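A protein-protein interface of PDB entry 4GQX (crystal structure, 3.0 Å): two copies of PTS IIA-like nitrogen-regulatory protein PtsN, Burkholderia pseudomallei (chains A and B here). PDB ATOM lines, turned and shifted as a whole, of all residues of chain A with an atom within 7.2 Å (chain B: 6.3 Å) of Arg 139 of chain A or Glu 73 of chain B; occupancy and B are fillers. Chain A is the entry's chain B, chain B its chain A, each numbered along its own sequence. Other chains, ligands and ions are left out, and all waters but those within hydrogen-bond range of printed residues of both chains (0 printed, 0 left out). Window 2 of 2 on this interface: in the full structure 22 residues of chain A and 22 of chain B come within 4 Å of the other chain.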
ATOM      1  N   GLU A  73     -30.199   0.448 -29.303  1.00  0.00           N
ATOM      2  CA  GLU A  73     -29.018   1.299 -29.411  1.00  0.00           C
ATOM      3  C   GLU A  73     -27.904   0.788 -30.388  1.00  0.00           C
ATOM      4  O   GLU A  73     -26.725   0.686 -30.022  1.00  0.00           O
ATOM      5  CB  GLU A  73     -28.435   1.567 -28.014  1.00  0.00           C
ATOM      6  CG  GLU A  73     -29.344   2.261 -27.033  1.00  0.00           C
ATOM      7  CD  GLU A  73     -28.698   2.334 -25.663  1.00  0.00           C
ATOM      8  OE1 GLU A  73     -28.929   3.315 -24.912  1.00  0.00           O
ATOM      9  OE2 GLU A  73     -27.930   1.399 -25.348  1.00  0.00           O
ATOM     10  N   GLN A 134     -24.970  -9.334 -22.603  1.00  0.00           N
ATOM     11  CA  GLN A 134     -24.628  -8.536 -21.455  1.00  0.00           C
ATOM     12  C   GLN A 134     -23.531  -7.553 -21.823  1.00  0.00           C
ATOM     13  O   GLN A 134     -23.470  -6.417 -21.315  1.00  0.00           O
ATOM     14  CB  GLN A 134     -24.154  -9.481 -20.387  1.00  0.00           C
ATOM     15  CG  GLN A 134     -23.646  -8.839 -19.177  1.00  0.00           C
ATOM     16  CD  GLN A 134     -23.380  -9.857 -18.140  1.00  0.00           C
ATOM     17  OE1 GLN A 134     -23.247  -9.545 -16.962  1.00  0.00           O
ATOM     18  NE2 GLN A 134     -23.316 -11.111 -18.561  1.00  0.00           N
ATOM     19  N   LEU A 135     -22.690  -8.021 -22.737  1.00  0.00           N
ATOM     20  CA  LEU A 135     -21.542  -7.288 -23.246  1.00  0.00           C
ATOM     21  C   LEU A 135     -21.967  -6.118 -24.131  1.00  0.00           C
ATOM     22  O   LEU A 135     -21.537  -4.986 -23.937  1.00  0.00           O
ATOM     23  CB  LEU A 135     -20.632  -8.259 -24.013  1.00  0.00           C
ATOM     24  CG  LEU A 135     -19.660  -7.742 -25.067  1.00  0.00           C
ATOM     25  CD1 LEU A 135     -18.625  -6.814 -24.474  1.00  0.00           C
ATOM     26  CD2 LEU A 135     -18.987  -8.936 -25.661  1.00  0.00           C
ATOM     27  N   LEU A 136     -22.812  -6.407 -25.109  1.00  0.00           N
ATOM     28  CA  LEU A 136     -23.351  -5.385 -25.988  1.00  0.00           C
ATOM     29  C   LEU A 136     -24.252  -4.418 -25.224  1.00  0.00           C
ATOM     30  O   LEU A 136     -24.262  -3.217 -25.490  1.00  0.00           O
ATOM     31  CB  LEU A 136     -24.138  -6.067 -27.093  1.00  0.00           C
ATOM     32  CG  LEU A 136     -23.303  -6.901 -28.056  1.00  0.00           C
ATOM     33  CD1 LEU A 136     -24.217  -7.808 -28.880  1.00  0.00           C
ATOM     34  CD2 LEU A 136     -22.473  -5.971 -28.949  1.00  0.00           C
ATOM     35  N   SER A 137     -24.996  -4.972 -24.267  1.00  0.00           N
ATOM     36  CA  SER A 137     -25.958  -4.242 -23.460  1.00  0.00           C
ATOM     37  C   SER A 137     -25.302  -3.127 -22.654  1.00  0.00           C
ATOM     38  O   SER A 137     -25.815  -2.001 -22.628  1.00  0.00           O
ATOM     39  CB  SER A 137     -26.694  -5.198 -22.533  1.00  0.00           C
ATOM     40  OG  SER A 137     -27.482  -4.495 -21.595  1.00  0.00           O
ATOM     41  N   ASP A 138     -24.181  -3.422 -21.998  1.00  0.00           N
ATOM     42  CA  ASP A 138     -23.480  -2.385 -21.242  1.00  0.00           C
ATOM     43  C   ASP A 138     -22.925  -1.270 -22.142  1.00  0.00           C
ATOM     44  O   ASP A 138     -22.136  -1.551 -23.032  1.00  0.00           O
ATOM     45  CB  ASP A 138     -22.352  -2.984 -20.423  1.00  0.00           C
ATOM     46  CG  ASP A 138     -21.647  -1.947 -19.603  1.00  0.00           C
ATOM     47  OD1 ASP A 138     -20.768  -1.260 -20.159  1.00  0.00           O
ATOM     48  OD2 ASP A 138     -21.992  -1.808 -18.410  1.00  0.00           O
ATOM     49  N   ARG A 139     -23.311  -0.016 -21.887  1.00  0.00           N
ATOM     50  CA  ARG A 139     -23.025   1.094 -22.815  1.00  0.00           C
ATOM     51  C   ARG A 139     -21.646   1.747 -22.670  1.00  0.00           C
ATOM     52  O   ARG A 139     -21.158   2.401 -23.597  1.00  0.00           O
ATOM     53  CB  ARG A 139     -24.141   2.151 -22.796  1.00  0.00           C
ATOM     54  CG  ARG A 139     -24.107   3.131 -21.634  1.00  0.00           C
ATOM     55  CD  ARG A 139     -24.801   4.446 -22.023  1.00  0.00           C
ATOM     56  NE  ARG A 139     -25.620   4.991 -20.932  1.00  0.00           N
ATOM     57  CZ  ARG A 139     -26.914   4.718 -20.740  1.00  0.00           C
ATOM     58  NH1 ARG A 139     -27.566   3.903 -21.572  1.00  0.00           N
ATOM     59  NH2 ARG A 139     -27.559   5.263 -19.714  1.00  0.00           N
ATOM     60  N   ASP A 140     -21.032   1.571 -21.506  1.00  0.00           N
ATOM     61  CA  ASP A 140     -19.632   1.921 -21.319  1.00  0.00           C
ATOM     62  C   ASP A 140     -18.804   1.157 -22.366  1.00  0.00           C
ATOM     63  O   ASP A 140     -17.905   1.711 -22.973  1.00  0.00           O
ATOM     64  CB  ASP A 140     -19.199   1.554 -19.889  1.00  0.00           C
ATOM     65  CG  ASP A 140     -18.213   2.553 -19.278  1.00  0.00           C
ATOM     66  OD1 ASP A 140     -18.436   3.778 -19.385  1.00  0.00           O
ATOM     67  OD2 ASP A 140     -17.227   2.107 -18.650  1.00  0.00           O
ATOM     68  N   THR A 141     -19.146  -0.112 -22.587  1.00  0.00           N
ATOM     69  CA  THR A 141     -18.452  -0.998 -23.529  1.00  0.00           C
ATOM     70  C   THR A 141     -18.896  -0.699 -24.948  1.00  0.00           C
ATOM     71  O   THR A 141     -18.072  -0.534 -25.843  1.00  0.00           O
ATOM     72  CB  THR A 141     -18.747  -2.485 -23.210  1.00  0.00           C
ATOM     73  OG1 THR A 141     -18.583  -2.715 -21.808  1.00  0.00           O
ATOM     74  CG2 THR A 141     -17.813  -3.390 -23.953  1.00  0.00           C
ATOM     75  N   ARG A 142     -20.213  -0.635 -25.128  1.00  0.00           N
ATOM     76  CA  ARG A 142     -20.870  -0.300 -26.387  1.00  0.00           C
ATOM     77  C   ARG A 142     -20.154   0.851 -27.101  1.00  0.00           C
ATOM     78  O   ARG A 142     -19.969   0.803 -28.313  1.00  0.00           O
ATOM     79  CB  ARG A 142     -22.336   0.056 -26.105  1.00  0.00           C
ATOM     80  CG  ARG A 142     -23.314  -0.084 -27.268  1.00  0.00           C
ATOM     81  CD  ARG A 142     -24.779   0.264 -26.870  1.00  0.00           C
ATOM     82  NE  ARG A 142     -24.898   1.606 -26.278  1.00  0.00           N
ATOM     83  CZ  ARG A 142     -24.979   2.768 -26.952  1.00  0.00           C
ATOM     84  NH1 ARG A 142     -24.978   2.798 -28.282  1.00  0.00           N
ATOM     85  NH2 ARG A 142     -25.062   3.921 -26.287  1.00  0.00           N
ATOM     86  N   GLU A 143     -19.739   1.873 -26.347  1.00  0.00           N
ATOM     87  CA  GLU A 143     -18.973   2.999 -26.905  1.00  0.00           C
ATOM     88  C   GLU A 143     -17.569   2.604 -27.372  1.00  0.00           C
ATOM     89  O   GLU A 143     -17.164   3.013 -28.454  1.00  0.00           O
ATOM     90  CB  GLU A 143     -18.886   4.168 -25.923  1.00  0.00           C
ATOM     91  CG  GLU A 143     -20.161   4.996 -25.801  1.00  0.00           C
ATOM     92  CD  GLU A 143     -20.056   6.116 -24.742  1.00  0.00           C
ATOM     93  OE1 GLU A 143     -20.881   6.133 -23.796  1.00  0.00           O
ATOM     94  OE2 GLU A 143     -19.149   6.978 -24.850  1.00  0.00           O
ATOM     95  N   ARG A 144     -16.839   1.816 -26.574  1.00  0.00           N
ATOM     96  CA  ARG A 144     -15.480   1.378 -26.938  1.00  0.00           C
ATOM     97  C   ARG A 144     -15.475   0.623 -28.247  1.00  0.00           C
ATOM     98  O   ARG A 144     -14.561   0.785 -29.043  1.00  0.00           O
ATOM     99  CB  ARG A 144     -14.846   0.507 -25.854  1.00  0.00           C
ATOM    100  CG  ARG A 144     -14.215   1.287 -24.705  1.00  0.00           C
ATOM    101  CD  ARG A 144     -13.932   0.407 -23.455  1.00  0.00           C
ATOM    102  NE  ARG A 144     -13.751   1.215 -22.233  1.00  0.00           N
ATOM    103  CZ  ARG A 144     -14.632   1.318 -21.225  1.00  0.00           C
ATOM    104  NH1 ARG A 144     -15.785   0.649 -21.245  1.00  0.00           N
ATOM    105  NH2 ARG A 144     -14.357   2.088 -20.174  1.00  0.00           N
ATOM    106  N   LEU B  71     -27.592  -6.987 -15.994  1.00  0.00           N
ATOM    107  CA  LEU B  71     -27.512  -6.648 -17.407  1.00  0.00           C
ATOM    108  C   LEU B  71     -27.143  -5.173 -17.607  1.00  0.00           C
ATOM    109  O   LEU B  71     -26.899  -4.722 -18.736  1.00  0.00           O
ATOM    110  CB  LEU B  71     -28.821  -7.003 -18.113  1.00  0.00           C
ATOM    111  CG  LEU B  71     -28.800  -7.271 -19.617  1.00  0.00           C
ATOM    112  CD1 LEU B  71     -28.479  -8.712 -19.900  1.00  0.00           C
ATOM    113  CD2 LEU B  71     -30.145  -6.911 -20.204  1.00  0.00           C
ATOM    114  N   GLY B  72     -27.069  -4.433 -16.501  1.00  0.00           N
ATOM    115  CA  GLY B  72     -26.825  -2.983 -16.555  1.00  0.00           C
ATOM    116  C   GLY B  72     -28.104  -2.235 -16.223  1.00  0.00           C
ATOM    117  O   GLY B  72     -29.209  -2.710 -16.544  1.00  0.00           O
ATOM    118  N   GLU B  73     -27.970  -1.097 -15.549  1.00  0.00           N
ATOM    119  CA  GLU B  73     -29.117  -0.250 -15.247  1.00  0.00           C
ATOM    120  C   GLU B  73     -30.247  -0.927 -14.412  1.00  0.00           C
ATOM    121  O   GLU B  73     -31.426  -0.919 -14.802  1.00  0.00           O
ATOM    122  CB  GLU B  73     -29.690   0.326 -16.545  1.00  0.00           C
ATOM    123  CG  GLU B  73     -28.764   1.188 -17.350  1.00  0.00           C
ATOM    124  CD  GLU B  73     -29.410   1.581 -18.652  1.00  0.00           C
ATOM    125  OE1 GLU B  73     -29.115   2.680 -19.176  1.00  0.00           O
ATOM    126  OE2 GLU B  73     -30.239   0.785 -19.144  1.00  0.00           O
ATOM    127  N   GLY B  74     -29.892  -1.504 -13.264  1.00  0.00           N
ATOM    128  CA  GLY B  74     -30.896  -2.044 -12.323  1.00  0.00           C
ATOM    129  C   GLY B  74     -31.554  -3.353 -12.745  1.00  0.00           C
ATOM    130  O   GLY B  74     -32.479  -3.842 -12.092  1.00  0.00           O
ATOM    131  N   VAL B  75     -31.051  -3.926 -13.832  1.00  0.00           N
ATOM    132  CA  VAL B  75     -31.661  -5.069 -14.486  1.00  0.00           C
ATOM    133  C   VAL B  75     -30.752  -6.284 -14.328  1.00  0.00           C
ATOM    134  O   VAL B  75     -29.522  -6.201 -14.545  1.00  0.00           O
ATOM    135  CB  VAL B  75     -31.842  -4.773 -15.991  1.00  0.00           C
ATOM    136  CG1 VAL B  75     -32.281  -6.000 -16.716  1.00  0.00           C
ATOM    137  CG2 VAL B  75     -32.849  -3.701 -16.191  1.00  0.00           C
ATOM    138  N   ALA B 103     -23.277  -5.439 -10.889  1.00  0.00           N
ATOM    139  CA  ALA B 103     -23.668  -5.223 -12.268  1.00  0.00           C
ATOM    140  C   ALA B 103     -22.499  -4.649 -13.083  1.00  0.00           C
ATOM    141  O   ALA B 103     -21.607  -4.018 -12.512  1.00  0.00           O
ATOM    142  CB  ALA B 103     -24.855  -4.290 -12.307  1.00  0.00           C
ATOM    143  N   ASP B 105     -22.194  -2.089 -14.928  1.00  0.00           N
ATOM    144  CA  ASP B 105     -22.058  -0.635 -14.843  1.00  0.00           C
ATOM    145  C   ASP B 105     -21.922  -0.100 -13.422  1.00  0.00           C
ATOM    146  O   ASP B 105     -21.934   1.105 -13.217  1.00  0.00           O
ATOM    147  CB  ASP B 105     -23.230   0.060 -15.543  1.00  0.00           C
ATOM    148  CG  ASP B 105     -24.570  -0.329 -14.960  1.00  0.00           C
ATOM    149  OD1 ASP B 105     -24.647  -1.357 -14.253  1.00  0.00           O
ATOM    150  OD2 ASP B 105     -25.554   0.393 -15.217  1.00  0.00           O
ATOM    151  N   GLN B 107     -24.002   0.042 -11.079  1.00  0.00           N
ATOM    152  CA  GLN B 107     -25.310   0.390 -10.507  1.00  0.00           C
ATOM    153  C   GLN B 107     -25.979  -0.760  -9.719  1.00  0.00           C
ATOM    154  O   GLN B 107     -25.829  -1.920 -10.090  1.00  0.00           O
ATOM    155  CB  GLN B 107     -26.256   0.855 -11.624  1.00  0.00           C
ATOM    156  CG  GLN B 107     -25.907   2.203 -12.267  1.00  0.00           C
ATOM    157  CD  GLN B 107     -27.033   2.769 -13.158  1.00  0.00           C
ATOM    158  OE1 GLN B 107     -28.104   2.172 -13.300  1.00  0.00           O
ATOM    159  NE2 GLN B 107     -26.784   3.933 -13.748  1.00  0.00           N
ATOM    160  N   PRO B 108     -26.745  -0.432  -8.648  1.00  0.00           N
ATOM    161  CA  PRO B 108     -27.572  -1.430  -7.939  1.00  0.00           C
ATOM    162  C   PRO B 108     -28.776  -1.958  -8.760  1.00  0.00           C
ATOM    163  O   PRO B 108     -29.247  -1.280  -9.684  1.00  0.00           O
ATOM    164  CB  PRO B 108     -28.058  -0.663  -6.702  1.00  0.00           C
ATOM    165  CG  PRO B 108     -28.085   0.753  -7.137  1.00  0.00           C
ATOM    166  CD  PRO B 108     -26.884   0.906  -8.038  1.00  0.00           C
ATOM    167  N   VAL B 109     -29.265  -3.150  -8.413  1.00  0.00           N
ATOM    168  CA  VAL B 109     -30.315  -3.821  -9.189  1.00  0.00           C
ATOM    169  C   VAL B 109     -31.645  -3.800  -8.436  1.00  0.00           C
ATOM    170  O   VAL B 109     -31.675  -4.101  -7.247  1.00  0.00           O
ATOM    171  CB  VAL B 109     -29.894  -5.289  -9.588  1.00  0.00           C
ATOM    172  CG1 VAL B 109     -31.061  -6.079 -10.127  1.00  0.00           C
ATOM    173  CG2 VAL B 109     -28.780  -5.298 -10.638  1.00  0.00           C
ATOM    174  N   LEU B 111     -34.819  -4.316 -10.636  1.00  0.00           N
ATOM    175  CA  LEU B 111     -35.608  -5.169 -11.523  1.00  0.00           C
ATOM    176  C   LEU B 111     -34.861  -6.466 -11.867  1.00  0.00           C
ATOM    177  O   LEU B 111     -33.700  -6.425 -12.300  1.00  0.00           O
ATOM    178  CB  LEU B 111     -35.917  -4.423 -12.821  1.00  0.00           C
ATOM    179  CG  LEU B 111     -36.832  -3.227 -12.698  1.00  0.00           C
ATOM    180  CD1 LEU B 111     -36.897  -2.515 -14.034  1.00  0.00           C
ATOM    181  CD2 LEU B 111     -38.191  -3.687 -12.261  1.00  0.00           C
ATOM    182  N   LEU B 136     -35.611  -6.598 -21.086  1.00  0.00           N
ATOM    183  CA  LEU B 136     -35.038  -5.810 -20.013  1.00  0.00           C
ATOM    184  C   LEU B 136     -34.104  -4.739 -20.558  1.00  0.00           C
ATOM    185  O   LEU B 136     -34.048  -3.623 -20.043  1.00  0.00           O
ATOM    186  CB  LEU B 136     -34.274  -6.739 -19.081  1.00  0.00           C
ATOM    187  CG  LEU B 136     -35.134  -7.754 -18.331  1.00  0.00           C
ATOM    188  CD1 LEU B 136     -34.248  -8.833 -17.706  1.00  0.00           C
ATOM    189  CD2 LEU B 136     -35.968  -7.035 -17.284  1.00  0.00           C
ATOM    190  N   SER B 137     -33.384  -5.105 -21.617  1.00  0.00           N
ATOM    191  CA  SER B 137     -32.392  -4.251 -22.252  1.00  0.00           C
ATOM    192  C   SER B 137     -32.996  -2.952 -22.785  1.00  0.00           C
ATOM    193  O   SER B 137     -32.440  -1.871 -22.550  1.00  0.00           O
ATOM    194  CB  SER B 137     -31.687  -5.011 -23.370  1.00  0.00           C
ATOM    195  OG  SER B 137     -30.841  -4.160 -24.113  1.00  0.00           O
ATOM    196  N   ARG B 139     -34.872   0.337 -22.853  1.00  0.00           N
ATOM    197  CA  ARG B 139     -35.103   1.228 -21.695  1.00  0.00           C
ATOM    198  C   ARG B 139     -36.450   1.955 -21.689  1.00  0.00           C
ATOM    199  O   ARG B 139     -36.902   2.438 -20.643  1.00  0.00           O
ATOM    200  CB  ARG B 139     -33.941   2.211 -21.487  1.00  0.00           C
ATOM    201  CG  ARG B 139     -33.938   3.432 -22.396  1.00  0.00           C
ATOM    202  CD  ARG B 139     -33.205   4.607 -21.729  1.00  0.00           C
ATOM    203  NE  ARG B 139     -32.356   5.346 -22.673  1.00  0.00           N
ATOM    204  CZ  ARG B 139     -31.074   5.068 -22.930  1.00  0.00           C
ATOM    205  NH1 ARG B 139     -30.458   4.062 -22.312  1.00  0.00           N
ATOM    206  NH2 ARG B 139     -30.401   5.800 -23.810  1.00  0.00           N
ATOM    207  N   ARG B 142     -37.984  -0.864 -19.805  1.00  0.00           N
ATOM    208  CA  ARG B 142     -37.322  -0.850 -18.508  1.00  0.00           C
ATOM    209  C   ARG B 142     -38.000   0.144 -17.564  1.00  0.00           C
ATOM    210  O   ARG B 142     -38.203  -0.162 -16.393  1.00  0.00           O
ATOM    211  CB  ARG B 142     -35.840  -0.504 -18.709  1.00  0.00           C
ATOM    212  CG  ARG B 142     -34.872  -0.931 -17.605  1.00  0.00           C
ATOM    213  CD  ARG B 142     -33.392  -0.556 -17.919  1.00  0.00           C
ATOM    214  NE  ARG B 142     -33.212   0.878 -18.205  1.00  0.00           N
ATOM    215  CZ  ARG B 142     -33.091   1.864 -17.294  1.00  0.00           C
ATOM    216  NH1 ARG B 142     -33.102   1.604 -15.989  1.00  0.00           N
ATOM    217  NH2 ARG B 142     -32.956   3.132 -17.686  1.00  0.00           N
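OE1 of Glu 73 of chain A lies within salt-bridge range of NH2 of Arg 139 of chain B, 3.1 Å away. The side-chain carboxylate of Glu 73 of chain B lies within salt-bridge range of the guanidinium group of Arg 139 of chain A (3.1 Å). The backbone carbonyl oxygen of Leu 71 of chain B sits at hydrogen-bond distance from the side-chain hydroxyl of Ser 137 of chain A. NH1 of Arg 139 of chain B lies close to NH1 of Arg 139 of chain A, at 3.0 Å. The backbone NH of Asp 105 of chain B lies within hydrogen-bond range of the side-chain carboxylate of Asp 138 of chain A, 3.5 Å away.
The guanidinium group (NE) of Arg 142 of chain B lies within salt-bridge range of the side-chain carboxylate (OE2) of Glu 73 of chain B (3.1 Å). The guanidinium group (NE) of Arg 142 of chain A is in salt-bridge range of the side-chain carboxylate (OE2) of Glu 73 of chain A, 3.2 Å away. The side-chain carboxylate of Glu 73 of chain A is in salt-bridge range of the guanidinium group of Arg 139 of chain A, 3.7 Å away. OD1 of Asp 138 of chain A sits at hydrogen-bond distance from N of Asp 140 of chain A (3.1 Å). The side-chain carboxylate of Asp 138 of chain A is in hydrogen-bond range of the side-chain hydroxyl of Thr 141 of chain A (3.1 Å). The backbone NH of Glu 73 of chain B is in hydrogen-bond range of the side-chain carboxylate of Asp 105 of chain B, 2.9 Å away.
Of chain B, only Glu 73 and Arg 139 come within 4 Å of Arg 139 of chain A. Of chain A, only Arg 139 comes within 4 Å of Glu 73 of chain B. Printed residues of chain B within 4 Å of Ser 137 of chain A: Leu 71. Printed residues of chain B within 4 Å of Glu 73 of chain A: Arg 139 (3.1 Å). Printed residues of chain A within 4 Å of Asp 105 of chain B: Asp 138. Ala 103 of chain B touches none of the printed residues of chain A. Arg 142 of chain A touches none of the printed residues of chain B. The nearest printed residue of chain B that does not touch Arg 139 of chain A is Arg 142 of chain B (6.1 Å). The nearest residue of chain A that does not touch Glu 73 of chain B is Glu 73 of chain A (5.8 Å).
Of the 15 printed residues of chain B, 4 touch a printed residue of chain A. Among the printed residues, 5 pairs touch across the chains. Among the printed residues, Asp or Glu carboxylates within 4 Å of a Lys or Arg side-chain nitrogen of the other chain: Glu 73 of chain A with Arg 139 of chain B (3.1 Å) and Arg 139 of chain A with Glu 73 of chain B (3.1 Å).
Glu 73 of chain A touches Arg 139 of chain B, and with the chains exchanged Arg 139 of chain A touches Glu 73 of chain B. Arg 139 of chain A touches its own counterpart, Arg 139 of chain B. Of the 5 pairs that touch across the chains among the printed residues, 3 have their exchanged pair printed and touching as well.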
